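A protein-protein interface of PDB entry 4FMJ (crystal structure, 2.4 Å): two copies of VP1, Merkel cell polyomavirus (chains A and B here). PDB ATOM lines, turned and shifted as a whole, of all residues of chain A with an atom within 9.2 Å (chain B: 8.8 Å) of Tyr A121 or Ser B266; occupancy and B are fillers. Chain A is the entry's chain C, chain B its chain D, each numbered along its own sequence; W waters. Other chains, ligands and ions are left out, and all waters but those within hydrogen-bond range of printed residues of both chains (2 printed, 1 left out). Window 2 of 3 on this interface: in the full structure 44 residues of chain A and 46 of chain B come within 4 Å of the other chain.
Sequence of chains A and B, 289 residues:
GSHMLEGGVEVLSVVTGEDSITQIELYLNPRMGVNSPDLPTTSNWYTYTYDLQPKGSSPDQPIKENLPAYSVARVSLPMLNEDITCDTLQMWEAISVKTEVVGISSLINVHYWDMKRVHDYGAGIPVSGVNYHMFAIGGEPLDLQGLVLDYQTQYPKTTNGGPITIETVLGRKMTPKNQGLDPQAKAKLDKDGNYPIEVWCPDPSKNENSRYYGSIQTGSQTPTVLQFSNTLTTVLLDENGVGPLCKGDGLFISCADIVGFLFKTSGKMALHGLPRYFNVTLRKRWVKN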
ATOM      1  N   VAL A 110      -7.560   6.187 -22.254  1.00  0.00           N
ATOM      2  CA  VAL A 110      -8.465   5.842 -21.154  1.00  0.00           C
ATOM      3  C   VAL A 110      -8.084   4.509 -20.489  1.00  0.00           C
ATOM      4  O   VAL A 110      -8.913   3.872 -19.823  1.00  0.00           O
ATOM      5  CB  VAL A 110      -9.948   5.808 -21.616  1.00  0.00           C
ATOM      6  CG1 VAL A 110     -10.459   7.223 -21.910  1.00  0.00           C
ATOM      7  CG2 VAL A 110     -10.138   4.881 -22.832  1.00  0.00           C
ATOM      8  N   LYS A 116      -8.510   5.952 -12.367  1.00  0.00           N
ATOM      9  CA  LYS A 116      -9.739   5.525 -11.700  1.00  0.00           C
ATOM     10  C   LYS A 116     -10.797   5.114 -12.717  1.00  0.00           C
ATOM     11  O   LYS A 116     -11.051   5.852 -13.662  1.00  0.00           O
ATOM     12  CB  LYS A 116     -10.276   6.648 -10.808  1.00  0.00           C
ATOM     13  CG  LYS A 116     -11.652   6.374 -10.238  1.00  0.00           C
ATOM     14  CD  LYS A 116     -11.874   7.118  -8.931  1.00  0.00           C
ATOM     15  CE  LYS A 116     -13.252   6.794  -8.335  1.00  0.00           C
ATOM     16  NZ  LYS A 116     -13.486   5.321  -8.136  1.00  0.00           N
ATOM     17  N   ARG A 117     -11.381   3.927 -12.529  1.00  0.00           N
ATOM     18  CA  ARG A 117     -12.434   3.410 -13.421  1.00  0.00           C
ATOM     19  C   ARG A 117     -13.736   4.194 -13.225  1.00  0.00           C
ATOM     20  O   ARG A 117     -14.121   4.496 -12.094  1.00  0.00           O
ATOM     21  CB  ARG A 117     -12.674   1.910 -13.194  1.00  0.00           C
ATOM     22  CG  ARG A 117     -11.460   0.999 -13.481  1.00  0.00           C
ATOM     23  CD  ARG A 117     -11.739  -0.473 -13.152  1.00  0.00           C
ATOM     24  NE  ARG A 117     -10.610  -1.359 -13.473  1.00  0.00           N
ATOM     25  CZ  ARG A 117     -10.515  -2.650 -13.132  1.00  0.00           C
ATOM     26  NH1 ARG A 117     -11.477  -3.256 -12.446  1.00  0.00           N
ATOM     27  NH2 ARG A 117      -9.443  -3.348 -13.479  1.00  0.00           N
ATOM     28  N   VAL A 118     -14.401   4.535 -14.327  1.00  0.00           N
ATOM     29  CA  VAL A 118     -15.663   5.290 -14.270  1.00  0.00           C
ATOM     30  C   VAL A 118     -16.702   4.585 -13.395  1.00  0.00           C
ATOM     31  O   VAL A 118     -17.300   5.201 -12.508  1.00  0.00           O
ATOM     32  CB  VAL A 118     -16.245   5.618 -15.678  1.00  0.00           C
ATOM     33  CG1 VAL A 118     -15.256   6.449 -16.481  1.00  0.00           C
ATOM     34  CG2 VAL A 118     -16.613   4.348 -16.450  1.00  0.00           C
ATOM     35  N   HIS A 119     -16.902   3.295 -13.655  1.00  0.00           N
ATOM     36  CA  HIS A 119     -17.675   2.413 -12.790  1.00  0.00           C
ATOM     37  C   HIS A 119     -16.941   1.063 -12.746  1.00  0.00           C
ATOM     38  O   HIS A 119     -15.948   0.884 -13.459  1.00  0.00           O
ATOM     39  CB  HIS A 119     -19.115   2.264 -13.308  1.00  0.00           C
ATOM     40  CG  HIS A 119     -19.212   1.861 -14.750  1.00  0.00           C
ATOM     41  ND1 HIS A 119     -19.839   2.641 -15.702  1.00  0.00           N
ATOM     42  CD2 HIS A 119     -18.764   0.759 -15.402  1.00  0.00           C
ATOM     43  CE1 HIS A 119     -19.778   2.031 -16.873  1.00  0.00           C
ATOM     44  NE2 HIS A 119     -19.127   0.891 -16.720  1.00  0.00           N
ATOM     45  N   ASP A 120     -17.417   0.126 -11.920  1.00  0.00           N
ATOM     46  CA  ASP A 120     -16.792  -1.200 -11.802  1.00  0.00           C
ATOM     47  C   ASP A 120     -16.554  -1.824 -13.175  1.00  0.00           C
ATOM     48  O   ASP A 120     -17.496  -1.973 -13.967  1.00  0.00           O
ATOM     49  CB  ASP A 120     -17.636  -2.151 -10.932  1.00  0.00           C
ATOM     50  CG  ASP A 120     -17.589  -1.804  -9.438  1.00  0.00           C
ATOM     51  OD1 ASP A 120     -17.092  -0.719  -9.072  1.00  0.00           O
ATOM     52  OD2 ASP A 120     -18.072  -2.627  -8.623  1.00  0.00           O
ATOM     53  N   TYR A 121     -15.285  -2.143 -13.449  1.00  0.00           N
ATOM     54  CA  TYR A 121     -14.852  -2.840 -14.668  1.00  0.00           C
ATOM     55  C   TYR A 121     -14.832  -2.014 -15.968  1.00  0.00           C
ATOM     56  O   TYR A 121     -14.566  -2.555 -17.055  1.00  0.00           O
ATOM     57  CB  TYR A 121     -15.644  -4.150 -14.857  1.00  0.00           C
ATOM     58  CG  TYR A 121     -15.750  -4.987 -13.588  1.00  0.00           C
ATOM     59  CD1 TYR A 121     -16.996  -5.402 -13.095  1.00  0.00           C
ATOM     60  CD2 TYR A 121     -14.610  -5.351 -12.874  1.00  0.00           C
ATOM     61  CE1 TYR A 121     -17.093  -6.174 -11.924  1.00  0.00           C
ATOM     62  CE2 TYR A 121     -14.695  -6.112 -11.702  1.00  0.00           C
ATOM     63  CZ  TYR A 121     -15.930  -6.523 -11.237  1.00  0.00           C
ATOM     64  OH  TYR A 121     -15.989  -7.270 -10.084  1.00  0.00           O
ATOM     65  N   GLY A 122     -15.086  -0.712 -15.856  1.00  0.00           N
ATOM     66  CA  GLY A 122     -15.094   0.172 -17.026  1.00  0.00           C
ATOM     67  C   GLY A 122     -13.780   0.884 -17.313  1.00  0.00           C
ATOM     68  O   GLY A 122     -12.794   0.709 -16.597  1.00  0.00           O
ATOM     69  N   ALA A 123     -13.769   1.695 -18.365  1.00  0.00           N
ATOM     70  CA  ALA A 123     -12.591   2.489 -18.731  1.00  0.00           C
ATOM     71  C   ALA A 123     -12.307   3.557 -17.683  1.00  0.00           C
ATOM     72  O   ALA A 123     -13.148   3.836 -16.839  1.00  0.00           O
ATOM     73  CB  ALA A 123     -12.776   3.123 -20.112  1.00  0.00           C
ATOM     74  N   GLY A 124     -11.118   4.147 -17.737  1.00  0.00           N
ATOM     75  CA  GLY A 124     -10.768   5.251 -16.851  1.00  0.00           C
ATOM     76  C   GLY A 124     -11.541   6.520 -17.179  1.00  0.00           C
ATOM     77  O   GLY A 124     -12.003   6.714 -18.299  1.00  0.00           O
ATOM     78  N   ASP B  51     -11.806  -4.285 -24.995  1.00  0.00           N
ATOM     79  CA  ASP B  51     -12.232  -3.614 -23.770  1.00  0.00           C
ATOM     80  C   ASP B  51     -11.103  -2.787 -23.163  1.00  0.00           C
ATOM     81  O   ASP B  51     -10.000  -3.282 -22.975  1.00  0.00           O
ATOM     82  CB  ASP B  51     -12.790  -4.626 -22.768  1.00  0.00           C
ATOM     83  CG  ASP B  51     -13.882  -5.514 -23.376  1.00  0.00           C
ATOM     84  OD1 ASP B  51     -13.649  -6.745 -23.465  1.00  0.00           O
ATOM     85  OD2 ASP B  51     -14.956  -4.989 -23.772  1.00  0.00           O
ATOM     86  N   LEU B  52     -11.391  -1.516 -22.883  1.00  0.00           N
ATOM     87  CA  LEU B  52     -10.421  -0.587 -22.303  1.00  0.00           C
ATOM     88  C   LEU B  52     -10.625  -0.530 -20.802  1.00  0.00           C
ATOM     89  O   LEU B  52     -11.681  -0.113 -20.318  1.00  0.00           O
ATOM     90  CB  LEU B  52     -10.574   0.805 -22.921  1.00  0.00           C
ATOM     91  CG  LEU B  52     -10.289   0.882 -24.430  1.00  0.00           C
ATOM     92  CD1 LEU B  52     -11.235   1.843 -25.113  1.00  0.00           C
ATOM     93  CD2 LEU B  52      -8.836   1.254 -24.714  1.00  0.00           C
ATOM     94  N   GLN B  53      -9.605  -0.955 -20.063  1.00  0.00           N
ATOM     95  CA  GLN B  53      -9.755  -1.190 -18.636  1.00  0.00           C
ATOM     96  C   GLN B  53      -8.438  -0.991 -17.883  1.00  0.00           C
ATOM     97  O   GLN B  53      -7.574  -1.866 -17.895  1.00  0.00           O
ATOM     98  CB  GLN B  53     -10.318  -2.601 -18.411  1.00  0.00           C
ATOM     99  CG  GLN B  53     -10.806  -2.892 -16.995  1.00  0.00           C
ATOM    100  CD  GLN B  53     -11.156  -4.367 -16.811  1.00  0.00           C
ATOM    101  OE1 GLN B  53     -10.267  -5.214 -16.676  1.00  0.00           O
ATOM    102  NE2 GLN B  53     -12.450  -4.680 -16.825  1.00  0.00           N
ATOM    103  N   PRO B  54      -8.276   0.174 -17.239  1.00  0.00           N
ATOM    104  CA  PRO B  54      -7.128   0.416 -16.366  1.00  0.00           C
ATOM    105  C   PRO B  54      -6.867  -0.778 -15.442  1.00  0.00           C
ATOM    106  O   PRO B  54      -7.773  -1.224 -14.728  1.00  0.00           O
ATOM    107  CB  PRO B  54      -7.571   1.629 -15.542  1.00  0.00           C
ATOM    108  CG  PRO B  54      -8.464   2.364 -16.448  1.00  0.00           C
ATOM    109  CD  PRO B  54      -9.188   1.333 -17.280  1.00  0.00           C
ATOM    110  N   ASP B 114     -26.096  -6.787 -25.830  1.00  0.00           N
ATOM    111  CA  ASP B 114     -25.291  -6.792 -24.609  1.00  0.00           C
ATOM    112  C   ASP B 114     -24.995  -5.384 -24.070  1.00  0.00           C
ATOM    113  O   ASP B 114     -23.936  -5.154 -23.463  1.00  0.00           O
ATOM    114  CB  ASP B 114     -23.986  -7.575 -24.835  1.00  0.00           C
ATOM    115  CG  ASP B 114     -23.310  -8.001 -23.528  1.00  0.00           C
ATOM    116  OD1 ASP B 114     -23.993  -8.077 -22.480  1.00  0.00           O
ATOM    117  OD2 ASP B 114     -22.089  -8.262 -23.547  1.00  0.00           O
ATOM    118  N   MET B 115     -25.931  -4.452 -24.277  1.00  0.00           N
ATOM    119  CA  MET B 115     -25.756  -3.053 -23.864  1.00  0.00           C
ATOM    120  C   MET B 115     -26.139  -2.895 -22.405  1.00  0.00           C
ATOM    121  O   MET B 115     -27.178  -3.405 -21.990  1.00  0.00           O
ATOM    122  CB  MET B 115     -26.643  -2.142 -24.713  1.00  0.00           C
ATOM    123  CG  MET B 115     -26.042  -0.792 -25.152  1.00  0.00           C
ATOM    124  SD  MET B 115     -27.024  -0.048 -26.499  1.00  0.00           S
ATOM    125  CE  MET B 115     -25.806   0.982 -27.311  1.00  0.00           C
ATOM    126  N   LYS B 116     -25.303  -2.199 -21.630  1.00  0.00           N
ATOM    127  CA  LYS B 116     -25.647  -1.810 -20.266  1.00  0.00           C
ATOM    128  C   LYS B 116     -26.826  -0.838 -20.280  1.00  0.00           C
ATOM    129  O   LYS B 116     -26.867   0.077 -21.100  1.00  0.00           O
ATOM    130  CB  LYS B 116     -24.449  -1.161 -19.559  1.00  0.00           C
ATOM    131  CG  LYS B 116     -24.731  -0.650 -18.127  1.00  0.00           C
ATOM    132  CD  LYS B 116     -23.444  -0.124 -17.490  1.00  0.00           C
ATOM    133  CE  LYS B 116     -23.674   0.515 -16.129  1.00  0.00           C
ATOM    134  NZ  LYS B 116     -23.968  -0.502 -15.081  1.00  0.00           N
ATOM    135  N   ARG B 117     -27.776  -1.046 -19.369  1.00  0.00           N
ATOM    136  CA  ARG B 117     -28.978  -0.205 -19.281  1.00  0.00           C
ATOM    137  C   ARG B 117     -28.722   1.088 -18.505  1.00  0.00           C
ATOM    138  O   ARG B 117     -27.912   1.114 -17.590  1.00  0.00           O
ATOM    139  CB  ARG B 117     -30.132  -0.976 -18.626  1.00  0.00           C
ATOM    140  CG  ARG B 117     -30.580  -2.258 -19.347  1.00  0.00           C
ATOM    141  CD  ARG B 117     -31.603  -3.024 -18.488  1.00  0.00           C
ATOM    142  NE  ARG B 117     -32.168  -4.189 -19.169  1.00  0.00           N
ATOM    143  CZ  ARG B 117     -33.371  -4.228 -19.735  1.00  0.00           C
ATOM    144  NH1 ARG B 117     -34.164  -3.167 -19.720  1.00  0.00           N
ATOM    145  NH2 ARG B 117     -33.787  -5.337 -20.326  1.00  0.00           N
ATOM    146  N   LEU B 262     -19.045   2.018 -26.573  1.00  0.00           N
ATOM    147  CA  LEU B 262     -20.074   0.999 -26.471  1.00  0.00           C
ATOM    148  C   LEU B 262     -20.043   0.432 -25.046  1.00  0.00           C
ATOM    149  O   LEU B 262     -19.088  -0.259 -24.680  1.00  0.00           O
ATOM    150  CB  LEU B 262     -19.843  -0.111 -27.493  1.00  0.00           C
ATOM    151  CG  LEU B 262     -20.962  -1.159 -27.552  1.00  0.00           C
ATOM    152  CD1 LEU B 262     -22.258  -0.574 -28.138  1.00  0.00           C
ATOM    153  CD2 LEU B 262     -20.528  -2.393 -28.331  1.00  0.00           C
ATOM    154  N   PHE B 263     -21.061   0.761 -24.246  1.00  0.00           N
ATOM    155  CA  PHE B 263     -21.192   0.285 -22.861  1.00  0.00           C
ATOM    156  C   PHE B 263     -21.828  -1.113 -22.824  1.00  0.00           C
ATOM    157  O   PHE B 263     -22.967  -1.307 -23.289  1.00  0.00           O
ATOM    158  CB  PHE B 263     -22.065   1.245 -22.040  1.00  0.00           C
ATOM    159  CG  PHE B 263     -21.426   2.571 -21.740  1.00  0.00           C
ATOM    160  CD1 PHE B 263     -21.370   3.572 -22.707  1.00  0.00           C
ATOM    161  CD2 PHE B 263     -20.905   2.832 -20.479  1.00  0.00           C
ATOM    162  CE1 PHE B 263     -20.787   4.791 -22.421  1.00  0.00           C
ATOM    163  CE2 PHE B 263     -20.326   4.058 -20.185  1.00  0.00           C
ATOM    164  CZ  PHE B 263     -20.263   5.035 -21.153  1.00  0.00           C
ATOM    165  N   LYS B 264     -21.104  -2.076 -22.265  1.00  0.00           N
ATOM    166  CA  LYS B 264     -21.578  -3.472 -22.189  1.00  0.00           C
ATOM    167  C   LYS B 264     -22.143  -3.841 -20.820  1.00  0.00           C
ATOM    168  O   LYS B 264     -21.809  -3.223 -19.809  1.00  0.00           O
ATOM    169  CB  LYS B 264     -20.455  -4.437 -22.548  1.00  0.00           C
ATOM    170  CG  LYS B 264     -20.021  -4.365 -24.003  1.00  0.00           C
ATOM    171  CD  LYS B 264     -18.604  -4.913 -24.164  1.00  0.00           C
ATOM    172  CE  LYS B 264     -18.059  -4.633 -25.539  1.00  0.00           C
ATOM    173  NZ  LYS B 264     -16.776  -5.344 -25.732  1.00  0.00           N
ATOM    174  N   THR B 265     -22.994  -4.863 -20.795  1.00  0.00           N
ATOM    175  CA  THR B 265     -23.674  -5.286 -19.559  1.00  0.00           C
ATOM    176  C   THR B 265     -22.721  -5.477 -18.361  1.00  0.00           C
ATOM    177  O   THR B 265     -23.047  -5.086 -17.246  1.00  0.00           O
ATOM    178  CB  THR B 265     -24.504  -6.570 -19.794  1.00  0.00           C
ATOM    179  OG1 THR B 265     -25.276  -6.421 -20.991  1.00  0.00           O
ATOM    180  CG2 THR B 265     -25.439  -6.870 -18.615  1.00  0.00           C
ATOM    181  N   SER B 266     -21.550  -6.065 -18.596  1.00  0.00           N
ATOM    182  CA  SER B 266     -20.607  -6.416 -17.515  1.00  0.00           C
ATOM    183  C   SER B 266     -19.942  -5.244 -16.788  1.00  0.00           C
ATOM    184  O   SER B 266     -19.410  -5.422 -15.694  1.00  0.00           O
ATOM    185  CB  SER B 266     -19.504  -7.309 -18.070  1.00  0.00           C
ATOM    186  OG  SER B 266     -18.864  -6.657 -19.156  1.00  0.00           O
ATOM    187  N   GLY B 267     -19.953  -4.062 -17.402  1.00  0.00           N
ATOM    188  CA  GLY B 267     -19.200  -2.908 -16.893  1.00  0.00           C
ATOM    189  C   GLY B 267     -18.171  -2.436 -17.908  1.00  0.00           C
ATOM    190  O   GLY B 267     -17.789  -1.262 -17.926  1.00  0.00           O
ATOM    191  N   LYS B 268     -17.757  -3.357 -18.777  1.00  0.00           N
ATOM    192  CA  LYS B 268     -16.723  -3.104 -19.781  1.00  0.00           C
ATOM    193  C   LYS B 268     -17.153  -2.115 -20.864  1.00  0.00           C
ATOM    194  O   LYS B 268     -18.341  -2.005 -21.203  1.00  0.00           O
ATOM    195  CB  LYS B 268     -16.263  -4.415 -20.433  1.00  0.00           C
ATOM    196  CG  LYS B 268     -15.599  -5.431 -19.479  1.00  0.00           C
ATOM    197  CD  LYS B 268     -15.090  -6.635 -20.265  1.00  0.00           C
ATOM    198  CE  LYS B 268     -14.857  -7.836 -19.399  1.00  0.00           C
ATOM    199  NZ  LYS B 268     -14.319  -8.974 -20.207  1.00  0.00           N
ATOM    200  N   MET B 269     -16.166  -1.421 -21.421  1.00  0.00           N
ATOM    201  CA  MET B 269     -16.401  -0.378 -22.427  1.00  0.00           C
ATOM    202  C   MET B 269     -15.368  -0.453 -23.537  1.00  0.00           C
ATOM    203  O   MET B 269     -14.169  -0.627 -23.276  1.00  0.00           O
ATOM    204  CB  MET B 269     -16.332   1.014 -21.780  1.00  0.00           C
ATOM    205  CG  MET B 269     -17.423   1.296 -20.763  1.00  0.00           C
ATOM    206  SD  MET B 269     -16.983   2.536 -19.526  1.00  0.00           S
ATOM    207  CE  MET B 269     -16.637   3.954 -20.582  1.00  0.00           C
ATOM    208  N   ALA B 270     -15.840  -0.311 -24.772  1.00  0.00           N
ATOM    209  CA  ALA B 270     -14.970  -0.262 -25.951  1.00  0.00           C
ATOM    210  C   ALA B 270     -15.238   1.009 -26.766  1.00  0.00           C
ATOM    211  O   ALA B 270     -16.372   1.486 -26.805  1.00  0.00           O
ATOM    212  CB  ALA B 270     -15.182  -1.491 -26.807  1.00  0.00           C
HETATM  213  O   HOH W   1     -13.918  -1.934 -19.728  1.00  0.00           O
HETATM  214  O   HOH W   2      -8.641  -0.133 -11.708  1.00  0.00           O
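NH2 of Arg A117 lies within hydrogen-bond range of O of Pro B54 (3.0 Å). A ring nitrogen (NE2) of His A119 sits at hydrogen-bond distance from the backbone carbonyl oxygen (O) of Gly B267 (2.8 Å). The side-chain amide nitrogen (NE2) of Gln B53 sits at hydrogen-bond distance from the backbone carbonyl oxygen (O) of Tyr A121. The backbone carbonyl oxygen (O) of Gly B267 sits close to the backbone NH (N) of Gly A122. The backbone NH of Ala A123 sits close to the backbone carbonyl oxygen of Leu B52 (3.4 Å). The backbone NH (N) of Ala A123 lies within hydrogen-bond range of the side-chain sulfur (SD) of Met B269, at 3.5 Å.
N of Gly A124 lies within hydrogen-bond range of O of Val A110, 3.0 Å away. The backbone carbonyl oxygen (O) of Ala A123 sits at hydrogen-bond distance from the backbone NH (N) of Val A118, 2.9 Å away. N of Leu B52 sits at hydrogen-bond distance from O of Met B269, at 2.9 Å. N of Lys B116 lies within hydrogen-bond range of O of Phe B263.
Among the printed residues, pairs that only touch across the chains: Gly A124 with Pro B54, Asp A120 with Gly B267, Tyr A121 with Lys B268, Tyr A121 with Ser B266, Tyr A121 with Gly B267, Val A118 with Met B269, Val A110 with Pro B54, Gly A122 with Pro B54, Arg A117 with Gln B53, Gly A122 with Leu B52, Ala A123 with Pro B54, His A119 with Phe B263, His A119 with Met B269, Gly A122 with Met B269 and Val A110 with Leu B52.
Printed residues of chain B within 4 Å of Val A118: Met B269 (3.6 Å). Printed residues of chain B within 4 Å of His A119: Phe B263 (3.9 Å), Gly B267 (2.8 Å) and Met B269 (3.9 Å). Of chain B, only Gln B53 (3.0 Å), Ser B266 (3.5 Å), Gly B267 (3.6 Å) and Lys B268 (3.5 Å) come within 4 Å of Tyr A121. Of the printed residues of chain A, Leu B52 touches Val A110, Gly A122 and Ala A123. Arg B117 touches none of the printed residues of chain A. Of the printed residues of chain A, Ser B266 touches Tyr A121 (3.5 Å). Of the printed residues of chain A, Lys B268 touches Tyr A121. Ala B270 touches none of the printed residues of chain A. The nearest residue of chain B that does not touch Tyr A121 is Met B269 (4.8 Å). The nearest residue of chain A that does not touch Ser B266 is Asp A120 (4.3 Å). The nearest printed residue of chain A that does not touch Pro B54 is Lys A116 (5.2 Å).
Hydrophobic or aromatic side chains of chain A that line the printed part of chain B: Val A110, Val A118, His A119, Tyr A121 and Ala A123. Hydrophobic or aromatic side chains of chain B within 4 Å of the printed part of chain A: Leu B52, Pro B54, Phe B263 and Met B269. Among the printed residues, no Asp or Glu carboxylate lies within 4 Å of a Lys or Arg side-chain nitrogen of the other chain.
2 positions are printed for both chains.
Water W1 lies within hydrogen-bond range of the backbone carbonyl oxygen of Tyr A121, the backbone NH of Met B269 and the backbone carbonyl oxygen of Leu B52. Water W2 bridges the guanidinium group (NE) of Arg A117 (2.9 Å) and the backbone carbonyl oxygen (O) of Pro B54 (3.3 Å).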
